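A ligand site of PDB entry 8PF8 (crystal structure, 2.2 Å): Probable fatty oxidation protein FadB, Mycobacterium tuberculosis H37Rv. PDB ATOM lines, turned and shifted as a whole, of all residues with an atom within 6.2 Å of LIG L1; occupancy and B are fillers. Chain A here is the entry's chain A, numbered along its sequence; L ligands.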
ATOM      1  N   HIS A   7      29.946  22.644 -15.589  1.00  0.00           N
ATOM      2  CA  HIS A   7      30.299  22.956 -16.997  1.00  0.00           C
ATOM      3  C   HIS A   7      31.760  23.400 -17.086  1.00  0.00           C
ATOM      4  O   HIS A   7      32.304  23.439 -18.219  1.00  0.00           O
ATOM      5  CB  HIS A   7      29.341  24.040 -17.518  1.00  0.00           C
ATOM      6  CG  HIS A   7      29.322  24.263 -18.991  1.00  0.00           C
ATOM      7  ND1 HIS A   7      29.569  23.248 -19.894  1.00  0.00           N
ATOM      8  CD2 HIS A   7      29.044  25.415 -19.681  1.00  0.00           C
ATOM      9  CE1 HIS A   7      29.460  23.804 -21.102  1.00  0.00           C
ATOM     10  NE2 HIS A   7      29.127  25.119 -21.017  1.00  0.00           N
ATOM     11  N   HIS A   8      32.370  23.741 -15.956  1.00  0.00           N
ATOM     12  CA  HIS A   8      33.771  24.174 -15.913  1.00  0.00           C
ATOM     13  C   HIS A   8      34.499  23.575 -14.700  1.00  0.00           C
ATOM     14  O   HIS A   8      33.933  23.524 -13.600  1.00  0.00           O
ATOM     15  CB  HIS A   8      33.873  25.700 -15.852  1.00  0.00           C
ATOM     16  CG  HIS A   8      33.086  26.400 -16.920  1.00  0.00           C
ATOM     17  ND1 HIS A   8      33.536  26.547 -18.211  1.00  0.00           N
ATOM     18  CD2 HIS A   8      31.878  27.008 -16.874  1.00  0.00           C
ATOM     19  CE1 HIS A   8      32.640  27.209 -18.913  1.00  0.00           C
ATOM     20  NE2 HIS A   8      31.622  27.506 -18.129  1.00  0.00           N
ATOM     21  N   MET A  46      17.234  26.006 -20.159  1.00  0.00           N
ATOM     22  CA  MET A  46      18.497  25.282 -19.969  1.00  0.00           C
ATOM     23  C   MET A  46      19.627  26.147 -20.490  1.00  0.00           C
ATOM     24  O   MET A  46      20.186  25.941 -21.567  1.00  0.00           O
ATOM     25  CB  MET A  46      18.455  23.930 -20.662  1.00  0.00           C
ATOM     26  CG  MET A  46      19.546  22.977 -20.188  1.00  0.00           C
ATOM     27  SD  MET A  46      19.049  21.253 -20.350  1.00  0.00           S
ATOM     28  CE  MET A  46      17.626  21.199 -19.252  1.00  0.00           C
ATOM     29  N   ASN A  47      19.980  27.155 -19.684  1.00  0.00           N
ATOM     30  CA  ASN A  47      21.078  28.058 -19.971  1.00  0.00           C
ATOM     31  C   ASN A  47      22.259  27.718 -19.069  1.00  0.00           C
ATOM     32  O   ASN A  47      22.209  26.791 -18.254  1.00  0.00           O
ATOM     33  CB  ASN A  47      20.634  29.516 -19.793  1.00  0.00           C
ATOM     34  CG  ASN A  47      19.951  29.762 -18.460  1.00  0.00           C
ATOM     35  OD1 ASN A  47      19.997  28.925 -17.557  1.00  0.00           O
ATOM     36  ND2 ASN A  47      19.296  30.911 -18.337  1.00  0.00           N
ATOM     37  N   GLU A  48      23.340  28.488 -19.218  1.00  0.00           N
ATOM     38  CA  GLU A  48      24.540  28.248 -18.426  1.00  0.00           C
ATOM     39  C   GLU A  48      24.269  28.425 -16.942  1.00  0.00           C
ATOM     40  O   GLU A  48      24.872  27.737 -16.110  1.00  0.00           O
ATOM     41  CB  GLU A  48      25.654  29.184 -18.896  1.00  0.00           C
ATOM     42  CG  GLU A  48      27.062  28.680 -18.620  1.00  0.00           C
ATOM     43  CD  GLU A  48      28.101  29.401 -19.441  1.00  0.00           C
ATOM     44  OE1 GLU A  48      27.735  30.322 -20.199  1.00  0.00           O
ATOM     45  OE2 GLU A  48      29.306  29.050 -19.330  1.00  0.00           O
ATOM     46  N   ALA A  49      23.363  29.333 -16.584  1.00  0.00           N
ATOM     47  CA  ALA A  49      23.037  29.551 -15.182  1.00  0.00           C
ATOM     48  C   ALA A  49      22.325  28.350 -14.575  1.00  0.00           C
ATOM     49  O   ALA A  49      22.585  27.989 -13.415  1.00  0.00           O
ATOM     50  CB  ALA A  49      22.178  30.816 -15.025  1.00  0.00           C
ATOM     51  N   ILE A  51      22.634  25.134 -15.527  1.00  0.00           N
ATOM     52  CA  ILE A  51      23.542  24.001 -15.409  1.00  0.00           C
ATOM     53  C   ILE A  51      24.388  24.117 -14.149  1.00  0.00           C
ATOM     54  O   ILE A  51      24.593  23.143 -13.423  1.00  0.00           O
ATOM     55  CB  ILE A  51      24.412  23.876 -16.673  1.00  0.00           C
ATOM     56  CG1 ILE A  51      23.533  23.603 -17.893  1.00  0.00           C
ATOM     57  CG2 ILE A  51      25.454  22.772 -16.498  1.00  0.00           C
ATOM     58  CD1 ILE A  51      24.314  23.400 -19.182  1.00  0.00           C
ATOM     59  N   GLY A  84      15.998  26.003 -24.164  1.00  0.00           N
ATOM     60  CA  GLY A  84      17.412  26.170 -23.914  1.00  0.00           C
ATOM     61  C   GLY A  84      17.877  27.490 -24.502  1.00  0.00           C
ATOM     62  O   GLY A  84      17.121  28.212 -25.151  1.00  0.00           O
ATOM     63  N   ASP A  85      19.156  27.787 -24.253  1.00  0.00           N
ATOM     64  CA  ASP A  85      19.786  28.979 -24.811  1.00  0.00           C
ATOM     65  C   ASP A  85      20.055  28.729 -26.291  1.00  0.00           C
ATOM     66  O   ASP A  85      20.979  27.992 -26.650  1.00  0.00           O
ATOM     67  CB  ASP A  85      21.075  29.308 -24.048  1.00  0.00           C
ATOM     68  CG  ASP A  85      21.552  30.720 -24.286  1.00  0.00           C
ATOM     69  OD1 ASP A  85      22.105  31.002 -25.363  1.00  0.00           O
ATOM     70  OD2 ASP A  85      21.357  31.567 -23.384  1.00  0.00           O
ATOM     71  N   VAL A  86      19.243  29.339 -27.155  1.00  0.00           N
ATOM     72  CA  VAL A  86      19.296  29.033 -28.577  1.00  0.00           C
ATOM     73  C   VAL A  86      20.491  29.685 -29.262  1.00  0.00           C
ATOM     74  O   VAL A  86      21.075  29.102 -30.177  1.00  0.00           O
ATOM     75  CB  VAL A  86      17.969  29.438 -29.239  1.00  0.00           C
ATOM     76  CG1 VAL A  86      18.011  29.185 -30.747  1.00  0.00           C
ATOM     77  CG2 VAL A  86      16.822  28.670 -28.618  1.00  0.00           C
ATOM     78  N   THR A  88      23.349  29.814 -28.234  1.00  0.00           N
ATOM     79  CA  THR A  88      24.465  28.898 -28.080  1.00  0.00           C
ATOM     80  C   THR A  88      24.423  27.790 -29.136  1.00  0.00           C
ATOM     81  O   THR A  88      25.427  27.530 -29.814  1.00  0.00           O
ATOM     82  CB  THR A  88      24.461  28.301 -26.670  1.00  0.00           C
ATOM     83  OG1 THR A  88      24.532  29.359 -25.701  1.00  0.00           O
ATOM     84  CG2 THR A  88      25.650  27.370 -26.482  1.00  0.00           C
ATOM     85  N   MET A  89      23.265  27.146 -29.279  1.00  0.00           N
ATOM     86  CA  MET A  89      23.164  26.009 -30.197  1.00  0.00           C
ATOM     87  C   MET A  89      23.311  26.442 -31.647  1.00  0.00           C
ATOM     88  O   MET A  89      23.968  25.747 -32.440  1.00  0.00           O
ATOM     89  CB  MET A  89      21.842  25.277 -29.985  1.00  0.00           C
ATOM     90  CG  MET A  89      21.731  24.509 -28.679  1.00  0.00           C
ATOM     91  SD  MET A  89      20.231  23.506 -28.574  1.00  0.00           S
ATOM     92  CE  MET A  89      18.959  24.768 -28.473  1.00  0.00           C
ATOM     93  N   ALA A  92      26.912  26.813 -32.747  1.00  0.00           N
ATOM     94  CA  ALA A  92      27.814  25.673 -32.619  1.00  0.00           C
ATOM     95  C   ALA A  92      28.240  25.182 -33.999  1.00  0.00           C
ATOM     96  O   ALA A  92      27.420  24.687 -34.773  1.00  0.00           O
ATOM     97  CB  ALA A  92      27.136  24.556 -31.839  1.00  0.00           C
ATOM     98  N   ASP A  96      32.877  22.479 -32.947  1.00  0.00           N
ATOM     99  CA  ASP A  96      32.417  22.544 -31.566  1.00  0.00           C
ATOM    100  C   ASP A  96      31.683  21.283 -31.125  1.00  0.00           C
ATOM    101  O   ASP A  96      31.093  21.265 -30.044  1.00  0.00           O
ATOM    102  CB  ASP A  96      31.505  23.764 -31.377  1.00  0.00           C
ATOM    103  CG  ASP A  96      32.197  25.065 -31.727  1.00  0.00           C
ATOM    104  OD1 ASP A  96      33.408  25.190 -31.439  1.00  0.00           O
ATOM    105  OD2 ASP A  96      31.532  25.962 -32.287  1.00  0.00           O
ATOM    106  N   ALA A  97      31.714  20.230 -31.946  1.00  0.00           N
ATOM    107  CA  ALA A  97      30.995  19.005 -31.616  1.00  0.00           C
ATOM    108  C   ALA A  97      31.493  18.382 -30.311  1.00  0.00           C
ATOM    109  O   ALA A  97      30.700  17.782 -29.578  1.00  0.00           O
ATOM    110  CB  ALA A  97      31.123  17.994 -32.759  1.00  0.00           C
ATOM    111  N   GLY A  98      32.789  18.525 -30.015  1.00  0.00           N
ATOM    112  CA  GLY A  98      33.293  18.015 -28.750  1.00  0.00           C
ATOM    113  C   GLY A  98      32.722  18.754 -27.546  1.00  0.00           C
ATOM    114  O   GLY A  98      32.419  18.129 -26.522  1.00  0.00           O
ATOM    115  N   ASP A  99      32.561  20.072 -27.665  1.00  0.00           N
ATOM    116  CA  ASP A  99      31.979  20.836 -26.567  1.00  0.00           C
ATOM    117  C   ASP A  99      30.471  20.609 -26.458  1.00  0.00           C
ATOM    118  O   ASP A  99      29.941  20.543 -25.345  1.00  0.00           O
ATOM    119  CB  ASP A  99      32.282  22.333 -26.744  1.00  0.00           C
ATOM    120  CG  ASP A  99      33.762  22.625 -26.696  1.00  0.00           C
ATOM    121  OD1 ASP A  99      34.514  21.815 -26.114  1.00  0.00           O
ATOM    122  OD2 ASP A  99      34.180  23.671 -27.240  1.00  0.00           O
ATOM    123  N   VAL A 100      29.777  20.495 -27.592  1.00  0.00           N
ATOM    124  CA  VAL A 100      28.366  20.139 -27.565  1.00  0.00           C
ATOM    125  C   VAL A 100      28.173  18.791 -26.894  1.00  0.00           C
ATOM    126  O   VAL A 100      27.290  18.607 -26.052  1.00  0.00           O
ATOM    127  CB  VAL A 100      27.779  20.151 -28.991  1.00  0.00           C
ATOM    128  CG1 VAL A 100      26.318  19.684 -28.970  1.00  0.00           C
ATOM    129  CG2 VAL A 100      27.880  21.529 -29.620  1.00  0.00           C
ATOM    130  N   PHE A 101      29.012  17.814 -27.257  1.00  0.00           N
ATOM    131  CA  PHE A 101      28.943  16.492 -26.656  1.00  0.00           C
ATOM    132  C   PHE A 101      29.180  16.557 -25.157  1.00  0.00           C
ATOM    133  O   PHE A 101      28.432  15.960 -24.366  1.00  0.00           O
ATOM    134  CB  PHE A 101      29.947  15.568 -27.347  1.00  0.00           C
ATOM    135  CG  PHE A 101      30.143  14.249 -26.665  1.00  0.00           C
ATOM    136  CD1 PHE A 101      29.260  13.205 -26.877  1.00  0.00           C
ATOM    137  CD2 PHE A 101      31.230  14.041 -25.824  1.00  0.00           C
ATOM    138  CE1 PHE A 101      29.448  11.984 -26.245  1.00  0.00           C
ATOM    139  CE2 PHE A 101      31.418  12.820 -25.192  1.00  0.00           C
ATOM    140  CZ  PHE A 101      30.520  11.794 -25.410  1.00  0.00           C
ATOM    141  N   THR A 103      28.736  19.065 -23.176  1.00  0.00           N
ATOM    142  CA  THR A 103      27.725  19.841 -22.478  1.00  0.00           C
ATOM    143  C   THR A 103      26.520  18.977 -22.123  1.00  0.00           C
ATOM    144  O   THR A 103      26.036  19.005 -20.991  1.00  0.00           O
ATOM    145  CB  THR A 103      27.299  21.047 -23.321  1.00  0.00           C
ATOM    146  OG1 THR A 103      28.445  21.868 -23.579  1.00  0.00           O
ATOM    147  CG2 THR A 103      26.250  21.876 -22.589  1.00  0.00           C
ATOM    148  N   ILE A 107      24.946  17.714 -18.551  1.00  0.00           N
ATOM    149  CA  ILE A 107      23.535  17.894 -18.210  1.00  0.00           C
ATOM    150  C   ILE A 107      22.931  16.573 -17.749  1.00  0.00           C
ATOM    151  O   ILE A 107      22.200  16.529 -16.748  1.00  0.00           O
ATOM    152  CB  ILE A 107      22.773  18.484 -19.412  1.00  0.00           C
ATOM    153  CG1 ILE A 107      23.226  19.916 -19.680  1.00  0.00           C
ATOM    154  CG2 ILE A 107      21.279  18.444 -19.167  1.00  0.00           C
ATOM    155  CD1 ILE A 107      22.624  20.522 -20.926  1.00  0.00           C
HETATM  156  C1  LIG L   1      23.642  25.790 -22.256  1.00  0.00           C
HETATM  157  C2  LIG L   1      27.298  28.860 -23.153  1.00  0.00           C
HETATM  158  C3  LIG L   1      29.541  25.064 -25.768  1.00  0.00           C
HETATM  159  C4  LIG L   1      28.633  25.392 -24.763  1.00  0.00           C
HETATM  160  C5  LIG L   1      29.423  25.699 -23.615  1.00  0.00           C
HETATM  161  C6  LIG L   1      29.275  24.659 -27.169  1.00  0.00           C
HETATM  162  C7  LIG L   1      31.952  25.733 -23.248  1.00  0.00           C
HETATM  163  N1  LIG L   1      26.712  27.590 -22.733  1.00  0.00           N
HETATM  164  N2  LIG L   1      25.351  27.475 -22.753  1.00  0.00           N
HETATM  165  C8  LIG L   1      27.289  26.443 -22.293  1.00  0.00           C
HETATM  166  N3  LIG L   1      30.719  25.551 -23.996  1.00  0.00           N
HETATM  167  C9  LIG L   1      25.060  26.241 -22.347  1.00  0.00           C
HETATM  168  O1  LIG L   1      29.576  27.458 -21.784  1.00  0.00           O
HETATM  169  C10 LIG L   1      26.226  25.530 -22.041  1.00  0.00           C
HETATM  170  N4  LIG L   1      30.794  25.155 -25.311  1.00  0.00           N
HETATM  171  B1  LIG L   1      28.895  26.154 -22.138  1.00  0.00           B
HETATM  172  F1  LIG L   1      22.833  26.516 -23.004  1.00  0.00           F
HETATM  173  F2  LIG L   1      23.489  24.536 -22.653  1.00  0.00           F
HETATM  174  F3  LIG L   1      23.166  25.835 -21.018  1.00  0.00           F
HETATM  175  F4  LIG L   1      28.119  25.125 -27.628  1.00  0.00           F
HETATM  176  F5  LIG L   1      30.209  25.080 -28.011  1.00  0.00           F
HETATM  177  F6  LIG L   1      29.209  23.346 -27.328  1.00  0.00           F
HETATM  178  N1  LG2 L   2      21.555  23.963 -25.164  1.00  0.00           N
HETATM  179  O1  LG2 L   2      18.885  22.369 -24.657  1.00  0.00           O
HETATM  180  C1  LG2 L   2      22.588  22.042 -25.496  1.00  0.00           C
HETATM  181  C2  LG2 L   2      24.833  23.120 -26.276  1.00  0.00           C
HETATM  182  C3  LG2 L   2      20.591  25.008 -24.861  1.00  0.00           C
HETATM  183  C4  LG2 L   2      23.421  23.130 -25.786  1.00  0.00           C
HETATM  184  F1  LG2 L   2      25.346  21.905 -26.292  1.00  0.00           F
HETATM  185  F2  LG2 L   2      24.934  23.581 -27.519  1.00  0.00           F
HETATM  186  F3  LG2 L   2      25.624  23.878 -25.535  1.00  0.00           F
HETATM  187  N2  LG2 L   2      22.809  24.295 -25.594  1.00  0.00           N
HETATM  188  C5  LG2 L   2      21.391  22.585 -25.097  1.00  0.00           C
HETATM  189  B1  LG2 L   2      20.120  21.799 -24.657  1.00  0.00           B
HETATM  190  O2  LG2 L   2      20.244  20.498 -24.273  1.00  0.00           O
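A boron (B1) of LIG L1 is covalently linked to a ring nitrogen (NE2) of His 7.
An oxygen (O1) of LIG L1 lies within hydrogen-bond range of the side-chain carboxylate (OE2) of Glu 48, at 2.9 Å.
The side-chain carboxylate (OE2) of Glu 48 sits at hydrogen-bond distance from a ring nitrogen (NE2) of His 8.
The backbone carbonyl oxygen (O) of Met 46 sits at hydrogen-bond distance from the backbone NH (N) of Asp 85, at 3.4 Å.
The backbone carbonyl oxygen (O) of Asp 99 lies within hydrogen-bond range of the side-chain hydroxyl (OG1) of Thr 103, at 2.7 Å.
The side-chain carboxylate (OD1) of Asp 85 sits at hydrogen-bond distance from the side-chain hydroxyl (OG1) of Thr 88 (3.0 Å).
The backbone carbonyl oxygen (O) of Met 46 sits close to a fluorine (F3) of LIG L1 (3.0 Å).
O of Asn 47 lies close to F3 of LIG L1, at 3.1 Å.
The backbone NH (N) of Val 100 sits close to a fluorine (F6) of LIG L1 (2.9 Å).
Residues that only touch LIG L1: Ile 51, Asp 85, Thr 88, Asp 96, Asp 99 and Thr 103.
Hydrophobic or aromatic side chains within 4 Å of LIG L1: His 7, Ile 51 and Val 100.
The nearest printed residue that does not touch LIG L1 is His 8 (4.2 Å).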
